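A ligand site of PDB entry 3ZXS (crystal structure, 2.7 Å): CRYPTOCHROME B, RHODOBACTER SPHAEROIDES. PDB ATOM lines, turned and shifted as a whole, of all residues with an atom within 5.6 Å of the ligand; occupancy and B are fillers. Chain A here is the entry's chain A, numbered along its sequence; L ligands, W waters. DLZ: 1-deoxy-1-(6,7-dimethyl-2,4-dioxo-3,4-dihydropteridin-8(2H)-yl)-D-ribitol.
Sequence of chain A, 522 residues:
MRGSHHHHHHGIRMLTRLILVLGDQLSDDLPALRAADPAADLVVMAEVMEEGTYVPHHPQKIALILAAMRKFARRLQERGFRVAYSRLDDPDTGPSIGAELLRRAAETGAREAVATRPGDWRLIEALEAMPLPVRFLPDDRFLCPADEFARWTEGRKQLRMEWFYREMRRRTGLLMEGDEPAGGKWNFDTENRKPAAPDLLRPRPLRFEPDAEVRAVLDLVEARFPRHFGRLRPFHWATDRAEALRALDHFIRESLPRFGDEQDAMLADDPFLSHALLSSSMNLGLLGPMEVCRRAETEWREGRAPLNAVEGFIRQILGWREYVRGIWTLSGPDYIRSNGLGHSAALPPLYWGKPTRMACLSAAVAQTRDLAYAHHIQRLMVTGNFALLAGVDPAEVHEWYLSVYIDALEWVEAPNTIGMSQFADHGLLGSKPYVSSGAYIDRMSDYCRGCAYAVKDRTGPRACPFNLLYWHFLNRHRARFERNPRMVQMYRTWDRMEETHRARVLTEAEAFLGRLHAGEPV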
ATOM      1  N   VAL A  21      -8.598   5.949 -18.989  1.00  0.00           N
ATOM      2  CA  VAL A  21      -8.901   7.273 -19.499  1.00  0.00           C
ATOM      3  C   VAL A  21     -10.183   7.793 -18.830  1.00  0.00           C
ATOM      4  O   VAL A  21     -11.270   7.300 -19.049  1.00  0.00           O
ATOM      5  CB  VAL A  21      -9.055   7.317 -21.022  1.00  0.00           C
ATOM      6  CG1 VAL A  21      -9.240   8.751 -21.480  1.00  0.00           C
ATOM      7  CG2 VAL A  21      -7.837   6.719 -21.702  1.00  0.00           C
ATOM      8  N   LEU A  22     -10.010   8.801 -17.985  1.00  0.00           N
ATOM      9  CA  LEU A  22     -11.134   9.404 -17.301  1.00  0.00           C
ATOM     10  C   LEU A  22     -11.804  10.373 -18.239  1.00  0.00           C
ATOM     11  O   LEU A  22     -11.324  10.637 -19.329  1.00  0.00           O
ATOM     12  CB  LEU A  22     -10.627  10.110 -16.057  1.00  0.00           C
ATOM     13  CG  LEU A  22     -10.147   9.136 -14.986  1.00  0.00           C
ATOM     14  CD1 LEU A  22      -9.265   9.852 -13.986  1.00  0.00           C
ATOM     15  CD2 LEU A  22     -11.348   8.414 -14.342  1.00  0.00           C
ATOM     16  N   GLY A  23     -12.917  10.918 -17.809  1.00  0.00           N
ATOM     17  CA  GLY A  23     -13.692  11.795 -18.672  1.00  0.00           C
ATOM     18  C   GLY A  23     -13.128  13.179 -18.955  1.00  0.00           C
ATOM     19  O   GLY A  23     -13.625  13.875 -19.855  1.00  0.00           O
ATOM     20  N   ASP A  24     -12.114  13.599 -18.224  1.00  0.00           N
ATOM     21  CA  ASP A  24     -11.478  14.845 -18.592  1.00  0.00           C
ATOM     22  C   ASP A  24     -10.119  14.628 -19.251  1.00  0.00           C
ATOM     23  O   ASP A  24      -9.290  15.531 -19.228  1.00  0.00           O
ATOM     24  CB  ASP A  24     -11.353  15.766 -17.385  1.00  0.00           C
ATOM     25  CG  ASP A  24     -10.410  15.243 -16.341  1.00  0.00           C
ATOM     26  OD1 ASP A  24     -10.339  13.994 -16.116  1.00  0.00           O
ATOM     27  OD2 ASP A  24      -9.758  16.090 -15.702  1.00  0.00           O
ATOM     28  N   GLN A  25      -9.917  13.444 -19.815  1.00  0.00           N
ATOM     29  CA  GLN A  25      -8.651  13.045 -20.360  1.00  0.00           C
ATOM     30  C   GLN A  25      -8.790  12.649 -21.849  1.00  0.00           C
ATOM     31  O   GLN A  25      -8.073  11.755 -22.360  1.00  0.00           O
ATOM     32  CB  GLN A  25      -8.112  11.887 -19.537  1.00  0.00           C
ATOM     33  CG  GLN A  25      -7.827  12.292 -18.085  1.00  0.00           C
ATOM     34  CD  GLN A  25      -7.137  11.205 -17.259  1.00  0.00           C
ATOM     35  OE1 GLN A  25      -7.236  10.026 -17.583  1.00  0.00           O
ATOM     36  NE2 GLN A  25      -6.467  11.611 -16.183  1.00  0.00           N
ATOM     37  N   ALA A  46     -15.122   4.384 -18.232  1.00  0.00           N
ATOM     38  CA  ALA A  46     -16.261   3.966 -17.380  1.00  0.00           C
ATOM     39  C   ALA A  46     -17.089   5.157 -16.971  1.00  0.00           C
ATOM     40  O   ALA A  46     -16.562   6.139 -16.430  1.00  0.00           O
ATOM     41  CB  ALA A  46     -15.785   3.216 -16.155  1.00  0.00           C
ATOM     42  N   GLU A  47     -18.382   5.047 -17.284  1.00  0.00           N
ATOM     43  CA  GLU A  47     -19.354   6.029 -16.908  1.00  0.00           C
ATOM     44  C   GLU A  47     -19.998   5.478 -15.639  1.00  0.00           C
ATOM     45  O   GLU A  47     -20.654   4.412 -15.684  1.00  0.00           O
ATOM     46  CB  GLU A  47     -20.422   6.155 -17.995  1.00  0.00           C
ATOM     47  CG  GLU A  47     -19.936   6.354 -19.426  1.00  0.00           C
ATOM     48  CD  GLU A  47     -21.091   6.402 -20.438  1.00  0.00           C
ATOM     49  OE1 GLU A  47     -22.197   5.870 -20.164  1.00  0.00           O
ATOM     50  OE2 GLU A  47     -20.893   6.979 -21.543  1.00  0.00           O
ATOM     51  N   VAL A  48     -19.833   6.181 -14.519  1.00  0.00           N
ATOM     52  CA  VAL A  48     -20.227   5.632 -13.206  1.00  0.00           C
ATOM     53  C   VAL A  48     -20.881   6.638 -12.284  1.00  0.00           C
ATOM     54  O   VAL A  48     -20.623   7.828 -12.343  1.00  0.00           O
ATOM     55  CB  VAL A  48     -19.010   4.996 -12.494  1.00  0.00           C
ATOM     56  CG1 VAL A  48     -18.398   3.893 -13.381  1.00  0.00           C
ATOM     57  CG2 VAL A  48     -17.961   6.037 -12.193  1.00  0.00           C
ATOM     58  N   GLU A  51     -18.959   9.263  -9.990  1.00  0.00           N
ATOM     59  CA  GLU A  51     -18.467  10.468 -10.619  1.00  0.00           C
ATOM     60  C   GLU A  51     -19.622  11.338 -11.051  1.00  0.00           C
ATOM     61  O   GLU A  51     -19.495  12.545 -11.203  1.00  0.00           O
ATOM     62  CB  GLU A  51     -17.560  10.114 -11.812  1.00  0.00           C
ATOM     63  CG  GLU A  51     -16.210   9.416 -11.427  1.00  0.00           C
ATOM     64  CD  GLU A  51     -15.470  10.112 -10.291  1.00  0.00           C
ATOM     65  OE1 GLU A  51     -15.096  11.305 -10.447  1.00  0.00           O
ATOM     66  OE2 GLU A  51     -15.278   9.457  -9.228  1.00  0.00           O
ATOM     67  N   GLY A  52     -20.782  10.752 -11.275  1.00  0.00           N
ATOM     68  CA  GLY A  52     -21.950  11.572 -11.572  1.00  0.00           C
ATOM     69  C   GLY A  52     -22.617  12.211 -10.384  1.00  0.00           C
ATOM     70  O   GLY A  52     -23.518  13.019 -10.555  1.00  0.00           O
ATOM     71  N   TYR A  54     -20.791  12.846  -6.943  1.00  0.00           N
ATOM     72  CA  TYR A  54     -19.967  13.340  -5.847  1.00  0.00           C
ATOM     73  C   TYR A  54     -20.283  14.806  -5.551  1.00  0.00           C
ATOM     74  O   TYR A  54     -20.196  15.256  -4.411  1.00  0.00           O
ATOM     75  CB  TYR A  54     -18.484  13.130  -6.112  1.00  0.00           C
ATOM     76  CG  TYR A  54     -17.839  13.913  -7.231  1.00  0.00           C
ATOM     77  CD1 TYR A  54     -17.775  13.399  -8.492  1.00  0.00           C
ATOM     78  CD2 TYR A  54     -17.212  15.120  -6.997  1.00  0.00           C
ATOM     79  CE1 TYR A  54     -17.128  14.087  -9.503  1.00  0.00           C
ATOM     80  CE2 TYR A  54     -16.567  15.818  -8.017  1.00  0.00           C
ATOM     81  CZ  TYR A  54     -16.535  15.307  -9.258  1.00  0.00           C
ATOM     82  OH  TYR A  54     -15.876  15.961 -10.276  1.00  0.00           O
ATOM     83  N   HIS A  57     -23.865  17.515 -10.253  1.00  0.00           N
ATOM     84  CA  HIS A  57     -23.419  18.311 -11.392  1.00  0.00           C
ATOM     85  C   HIS A  57     -24.611  18.800 -12.187  1.00  0.00           C
ATOM     86  O   HIS A  57     -25.664  18.141 -12.216  1.00  0.00           O
ATOM     87  CB  HIS A  57     -22.575  17.496 -12.382  1.00  0.00           C
ATOM     88  CG  HIS A  57     -21.399  16.793 -11.777  1.00  0.00           C
ATOM     89  ND1 HIS A  57     -20.152  17.375 -11.650  1.00  0.00           N
ATOM     90  CD2 HIS A  57     -21.264  15.536 -11.323  1.00  0.00           C
ATOM     91  CE1 HIS A  57     -19.314  16.511 -11.124  1.00  0.00           C
ATOM     92  NE2 HIS A  57     -19.964  15.381 -10.920  1.00  0.00           N
ATOM     93  N   LYS A  61     -23.402  19.457 -17.862  1.00  0.00           N
ATOM     94  CA  LYS A  61     -22.070  18.908 -17.599  1.00  0.00           C
ATOM     95  C   LYS A  61     -22.005  17.366 -17.655  1.00  0.00           C
ATOM     96  O   LYS A  61     -21.106  16.814 -18.305  1.00  0.00           O
ATOM     97  CB  LYS A  61     -21.474  19.418 -16.278  1.00  0.00           C
ATOM     98  CG  LYS A  61     -20.075  18.802 -16.016  1.00  0.00           C
ATOM     99  CD  LYS A  61     -19.216  19.560 -14.979  1.00  0.00           C
ATOM    100  CE  LYS A  61     -19.851  19.799 -13.631  1.00  0.00           C
ATOM    101  NZ  LYS A  61     -18.857  20.070 -12.525  1.00  0.00           N
ATOM    102  N   ILE A  62     -22.924  16.685 -16.978  1.00  0.00           N
ATOM    103  CA  ILE A  62     -22.917  15.239 -17.036  1.00  0.00           C
ATOM    104  C   ILE A  62     -23.037  14.779 -18.503  1.00  0.00           C
ATOM    105  O   ILE A  62     -22.287  13.950 -18.956  1.00  0.00           O
ATOM    106  CB  ILE A  62     -24.003  14.579 -16.185  1.00  0.00           C
ATOM    107  CG1 ILE A  62     -23.904  15.030 -14.711  1.00  0.00           C
ATOM    108  CG2 ILE A  62     -23.836  13.097 -16.247  1.00  0.00           C
ATOM    109  CD1 ILE A  62     -24.990  14.479 -13.771  1.00  0.00           C
ATOM    110  N   ILE A  65     -19.846  15.291 -20.663  1.00  0.00           N
ATOM    111  CA  ILE A  65     -18.732  14.369 -20.365  1.00  0.00           C
ATOM    112  C   ILE A  65     -19.020  12.988 -20.865  1.00  0.00           C
ATOM    113  O   ILE A  65     -18.197  12.393 -21.548  1.00  0.00           O
ATOM    114  CB  ILE A  65     -18.385  14.342 -18.882  1.00  0.00           C
ATOM    115  CG1 ILE A  65     -17.760  15.694 -18.502  1.00  0.00           C
ATOM    116  CG2 ILE A  65     -17.381  13.293 -18.602  1.00  0.00           C
ATOM    117  CD1 ILE A  65     -17.498  15.883 -17.066  1.00  0.00           C
ATOM    118  N   LEU A  66     -20.194  12.480 -20.571  1.00  0.00           N
ATOM    119  CA  LEU A  66     -20.516  11.138 -21.054  1.00  0.00           C
ATOM    120  C   LEU A  66     -20.465  11.071 -22.605  1.00  0.00           C
ATOM    121  O   LEU A  66     -19.891  10.133 -23.167  1.00  0.00           O
ATOM    122  CB  LEU A  66     -21.881  10.679 -20.523  1.00  0.00           C
ATOM    123  CG  LEU A  66     -21.858   9.957 -19.170  1.00  0.00           C
ATOM    124  CD1 LEU A  66     -20.973  10.649 -18.134  1.00  0.00           C
ATOM    125  CD2 LEU A  66     -23.275   9.752 -18.605  1.00  0.00           C
ATOM    126  N   MET A  69     -17.043  11.308 -23.929  1.00  0.00           N
ATOM    127  CA  MET A  69     -16.392  10.045 -23.576  1.00  0.00           C
ATOM    128  C   MET A  69     -16.648   8.972 -24.648  1.00  0.00           C
ATOM    129  O   MET A  69     -15.713   8.326 -25.106  1.00  0.00           O
ATOM    130  CB  MET A  69     -16.846   9.545 -22.199  1.00  0.00           C
ATOM    131  CG  MET A  69     -16.010  10.114 -21.052  1.00  0.00           C
ATOM    132  SD  MET A  69     -16.581   9.527 -19.450  1.00  0.00           S
ATOM    133  CE  MET A  69     -15.985   7.810 -19.516  1.00  0.00           C
ATOM    134  N   ILE A  97     -15.036   4.247 -10.553  1.00  0.00           N
ATOM    135  CA  ILE A  97     -13.942   3.966 -11.465  1.00  0.00           C
ATOM    136  C   ILE A  97     -13.139   2.772 -10.957  1.00  0.00           C
ATOM    137  O   ILE A  97     -12.710   1.924 -11.757  1.00  0.00           O
ATOM    138  CB  ILE A  97     -13.012   5.202 -11.661  1.00  0.00           C
ATOM    139  CG1 ILE A  97     -13.793   6.312 -12.350  1.00  0.00           C
ATOM    140  CG2 ILE A  97     -11.819   4.880 -12.527  1.00  0.00           C
ATOM    141  CD1 ILE A  97     -14.124   6.065 -13.817  1.00  0.00           C
ATOM    142  N   PRO A 118      -5.282  12.393 -12.226  1.00  0.00           N
ATOM    143  CA  PRO A 118      -6.467  13.238 -12.362  1.00  0.00           C
ATOM    144  C   PRO A 118      -6.370  14.558 -11.622  1.00  0.00           C
ATOM    145  O   PRO A 118      -5.412  14.802 -10.949  1.00  0.00           O
ATOM    146  CB  PRO A 118      -7.561  12.404 -11.713  1.00  0.00           C
ATOM    147  CG  PRO A 118      -6.927  11.097 -11.306  1.00  0.00           C
ATOM    148  CD  PRO A 118      -5.500  11.255 -11.322  1.00  0.00           C
ATOM    149  N   GLY A 119      -7.387  15.392 -11.748  1.00  0.00           N
ATOM    150  CA  GLY A 119      -7.355  16.701 -11.105  1.00  0.00           C
ATOM    151  C   GLY A 119      -8.406  16.859 -10.031  1.00  0.00           C
ATOM    152  O   GLY A 119      -9.102  17.865  -9.952  1.00  0.00           O
ATOM    153  N   ASP A 120      -8.507  15.833  -9.197  1.00  0.00           N
ATOM    154  CA  ASP A 120      -9.478  15.795  -8.126  1.00  0.00           C
ATOM    155  C   ASP A 120      -8.887  14.925  -7.030  1.00  0.00           C
ATOM    156  O   ASP A 120      -8.565  13.755  -7.284  1.00  0.00           O
ATOM    157  CB  ASP A 120     -10.774  15.222  -8.650  1.00  0.00           C
ATOM    158  CG  ASP A 120     -11.875  15.163  -7.579  1.00  0.00           C
ATOM    159  OD1 ASP A 120     -11.604  14.608  -6.514  1.00  0.00           O
ATOM    160  OD2 ASP A 120     -13.017  15.641  -7.797  1.00  0.00           O
ATOM    161  N   ARG A 122     -10.154  13.580  -4.231  1.00  0.00           N
ATOM    162  CA  ARG A 122     -10.944  12.433  -3.847  1.00  0.00           C
ATOM    163  C   ARG A 122     -10.714  11.275  -4.799  1.00  0.00           C
ATOM    164  O   ARG A 122     -10.551  10.131  -4.329  1.00  0.00           O
ATOM    165  CB  ARG A 122     -12.432  12.817  -3.833  1.00  0.00           C
ATOM    166  CG  ARG A 122     -13.456  11.675  -3.946  1.00  0.00           C
ATOM    167  CD  ARG A 122     -14.819  12.257  -4.362  1.00  0.00           C
ATOM    168  NE  ARG A 122     -14.750  12.803  -5.711  1.00  0.00           N
ATOM    169  CZ  ARG A 122     -14.826  12.084  -6.828  1.00  0.00           C
ATOM    170  NH1 ARG A 122     -14.977  10.783  -6.794  1.00  0.00           N
ATOM    171  NH2 ARG A 122     -14.752  12.662  -7.993  1.00  0.00           N
ATOM    172  N   LEU A 123     -10.697  11.557  -6.115  1.00  0.00           N
ATOM    173  CA  LEU A 123     -10.376  10.508  -7.091  1.00  0.00           C
ATOM    174  C   LEU A 123      -8.961  10.014  -6.933  1.00  0.00           C
ATOM    175  O   LEU A 123      -8.701   8.823  -7.021  1.00  0.00           O
ATOM    176  CB  LEU A 123     -10.591  10.968  -8.527  1.00  0.00           C
ATOM    177  CG  LEU A 123     -10.751   9.835  -9.541  1.00  0.00           C
ATOM    178  CD1 LEU A 123     -11.631   8.662  -9.050  1.00  0.00           C
ATOM    179  CD2 LEU A 123     -11.291  10.358 -10.846  1.00  0.00           C
ATOM    180  N   LEU A 409     -14.302  21.472 -12.672  1.00  0.00           N
ATOM    181  CA  LEU A 409     -13.638  20.308 -12.051  1.00  0.00           C
ATOM    182  C   LEU A 409     -12.800  20.825 -10.904  1.00  0.00           C
ATOM    183  O   LEU A 409     -12.411  21.984 -10.873  1.00  0.00           O
ATOM    184  CB  LEU A 409     -12.760  19.604 -13.049  1.00  0.00           C
ATOM    185  CG  LEU A 409     -13.406  19.244 -14.410  1.00  0.00           C
ATOM    186  CD1 LEU A 409     -12.317  19.012 -15.455  1.00  0.00           C
ATOM    187  CD2 LEU A 409     -14.311  18.021 -14.268  1.00  0.00           C
ATOM    188  N   GLU A 410     -12.526  19.978  -9.920  1.00  0.00           N
ATOM    189  CA  GLU A 410     -11.829  20.453  -8.720  1.00  0.00           C
ATOM    190  C   GLU A 410     -10.593  21.308  -8.975  1.00  0.00           C
ATOM    191  O   GLU A 410     -10.419  22.375  -8.356  1.00  0.00           O
ATOM    192  CB  GLU A 410     -11.404  19.311  -7.814  1.00  0.00           C
ATOM    193  CG  GLU A 410     -11.322  19.775  -6.334  1.00  0.00           C
ATOM    194  CD  GLU A 410     -10.615  18.757  -5.433  1.00  0.00           C
ATOM    195  OE1 GLU A 410      -9.505  18.262  -5.802  1.00  0.00           O
ATOM    196  OE2 GLU A 410     -11.183  18.457  -4.347  1.00  0.00           O
ATOM    197  N   TRP A 411      -9.718  20.871  -9.870  1.00  0.00           N
ATOM    198  CA  TRP A 411      -8.446  21.551  -9.984  1.00  0.00           C
ATOM    199  C   TRP A 411      -8.595  23.017 -10.369  1.00  0.00           C
ATOM    200  O   TRP A 411      -7.819  23.838  -9.918  1.00  0.00           O
ATOM    201  CB  TRP A 411      -7.464  20.814 -10.910  1.00  0.00           C
ATOM    202  CG  TRP A 411      -7.802  20.893 -12.342  1.00  0.00           C
ATOM    203  CD1 TRP A 411      -8.446  19.954 -13.075  1.00  0.00           C
ATOM    204  CD2 TRP A 411      -7.505  21.971 -13.213  1.00  0.00           C
ATOM    205  NE1 TRP A 411      -8.591  20.405 -14.365  1.00  0.00           N
ATOM    206  CE2 TRP A 411      -8.032  21.642 -14.471  1.00  0.00           C
ATOM    207  CE3 TRP A 411      -6.873  23.201 -13.039  1.00  0.00           C
ATOM    208  CZ2 TRP A 411      -7.949  22.506 -15.555  1.00  0.00           C
ATOM    209  CZ3 TRP A 411      -6.771  24.056 -14.116  1.00  0.00           C
ATOM    210  CH2 TRP A 411      -7.300  23.695 -15.364  1.00  0.00           C
HETATM  211  C7  DLZ L   1     -17.244  14.957 -14.167  1.00  0.00           C
HETATM  212  C7A DLZ L   1     -17.324  13.495 -14.525  1.00  0.00           C
HETATM  213  C5A DLZ L   1     -18.579  12.900 -14.573  1.00  0.00           C
HETATM  214  C6  DLZ L   1     -19.797  13.709 -14.229  1.00  0.00           C
HETATM  215  N5  DLZ L   1     -18.661  11.584 -14.876  1.00  0.00           N
HETATM  216  C4A DLZ L   1     -17.522  10.902 -15.144  1.00  0.00           C
HETATM  217  C4  DLZ L   1     -17.582   9.554 -15.464  1.00  0.00           C
HETATM  218  O4  DLZ L   1     -18.708   9.021 -15.471  1.00  0.00           O
HETATM  219  N3  DLZ L   1     -16.475   8.848 -15.779  1.00  0.00           N
HETATM  220  C2  DLZ L   1     -15.284   9.476 -15.775  1.00  0.00           C
HETATM  221  O2  DLZ L   1     -14.281   8.789 -16.076  1.00  0.00           O
HETATM  222  N1  DLZ L   1     -15.153  10.804 -15.462  1.00  0.00           N
HETATM  223  C8  DLZ L   1     -16.263  11.506 -15.130  1.00  0.00           C
HETATM  224  N8  DLZ L   1     -16.203  12.785 -14.797  1.00  0.00           N
HETATM  225  C1' DLZ L   1     -14.897  13.410 -14.783  1.00  0.00           C
HETATM  226  C2' DLZ L   1     -14.073  12.921 -13.584  1.00  0.00           C
HETATM  227  O2' DLZ L   1     -14.866  13.148 -12.413  1.00  0.00           O
HETATM  228  C3' DLZ L   1     -12.690  13.662 -13.625  1.00  0.00           C
HETATM  229  O3' DLZ L   1     -11.466  12.929 -13.894  1.00  0.00           O
HETATM  230  C4' DLZ L   1     -12.469  14.372 -12.338  1.00  0.00           C
HETATM  231  O4' DLZ L   1     -13.719  15.060 -12.006  1.00  0.00           O
HETATM  232  C5' DLZ L   1     -11.216  15.270 -12.586  1.00  0.00           C
HETATM  233  O5' DLZ L   1     -10.113  14.714 -13.339  1.00  0.00           O
HETATM  234  O   HOH W   1     -21.231   9.926 -14.287  1.00  0.00           O
HETATM  235  O   HOH W   2     -13.477  17.063 -10.069  1.00  0.00           O
HETATM  236  O   HOH W   3     -13.420   6.550 -17.431  1.00  0.00           O
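Residues that only touch the ligand: Ile 65, Glu 47, Leu 22, Ile 97, His 57, Leu 409, Pro 118, Leu 66, Asp 120 and Leu 123.
Hydrophobic or aromatic side chains that line the ligand: Leu 22, Tyr 54, His 57, Ile 65, Leu 66, Met 69, Ile 97, Pro 118, Leu 123 and Leu 409.
Of the 26 residues printed, 18 come within 4 Å of the ligand.
The nearest printed residue that does not touch the ligand is Gly 52 (4.03 Å).
Water W3 lies within hydrogen-bond range of O2 of the ligand, O of Val 21 and N of Ala 46.
Water W2 lies within hydrogen-bond range of OH of Tyr 54 (2.6 Å), OD2 of Asp 120 (2.7 Å), O4' of the ligand (2.8 Å) and N of Glu 410 (3.1 Å).
Water W1 lies within hydrogen-bond range of the backbone carbonyl oxygen of Val 48 (2.9 Å), an oxygen (O4) of the ligand (2.9 Å) and the backbone NH of Gly 52 (3.2 Å).
OE1 of Glu 51 lies within hydrogen-bond range of O2' of the ligand, 2.7 Å away.
The side-chain carboxylate (OD1) of Asp 24 sits at hydrogen-bond distance from an oxygen (O3') of the ligand, at 2.7 Å.
A nitrogen (N3) of the ligand sits at hydrogen-bond distance from the backbone carbonyl oxygen (O) of Ala 46.
OH of Tyr 54 is in hydrogen-bond range of O4' of the ligand.
N of Gly 23 lies within hydrogen-bond range of O2 of the ligand (3.1 Å).
N of Val 48 is in hydrogen-bond range of O4 of the ligand (3.2 Å).
O5' of the ligand lies within hydrogen-bond range of N of Gly 119 (3.2 Å).
SD of Met 69 is in hydrogen-bond range of N3 of the ligand (3.7 Å).
The backbone carbonyl oxygen of Glu 51 is in hydrogen-bond range of a ring nitrogen (NE2) of His 57, 2.9 Å away.
The guanidinium group of Arg 122 is in salt-bridge range of the side-chain carboxylate of Glu 51.
The backbone NH (N) of Trp 411 lies within hydrogen-bond range of the backbone carbonyl oxygen (O) of Gly 119.
The backbone NH (N) of Leu 22 sits at hydrogen-bond distance from the side-chain amide oxygen (OE1) of Gln 25 (3.1 Å).
A ring nitrogen (ND1) of His 57 lies within hydrogen-bond range of the side-chain amino group of Lys 61 (3.1 Å).
N of Leu 123 sits at hydrogen-bond distance from OD1 of Asp 120, at 3.2 Å.
The side-chain carboxylate (OD2) of Asp 120 is in salt-bridge range of the guanidinium group (NH2) of Arg 122, at 3.5 Å.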
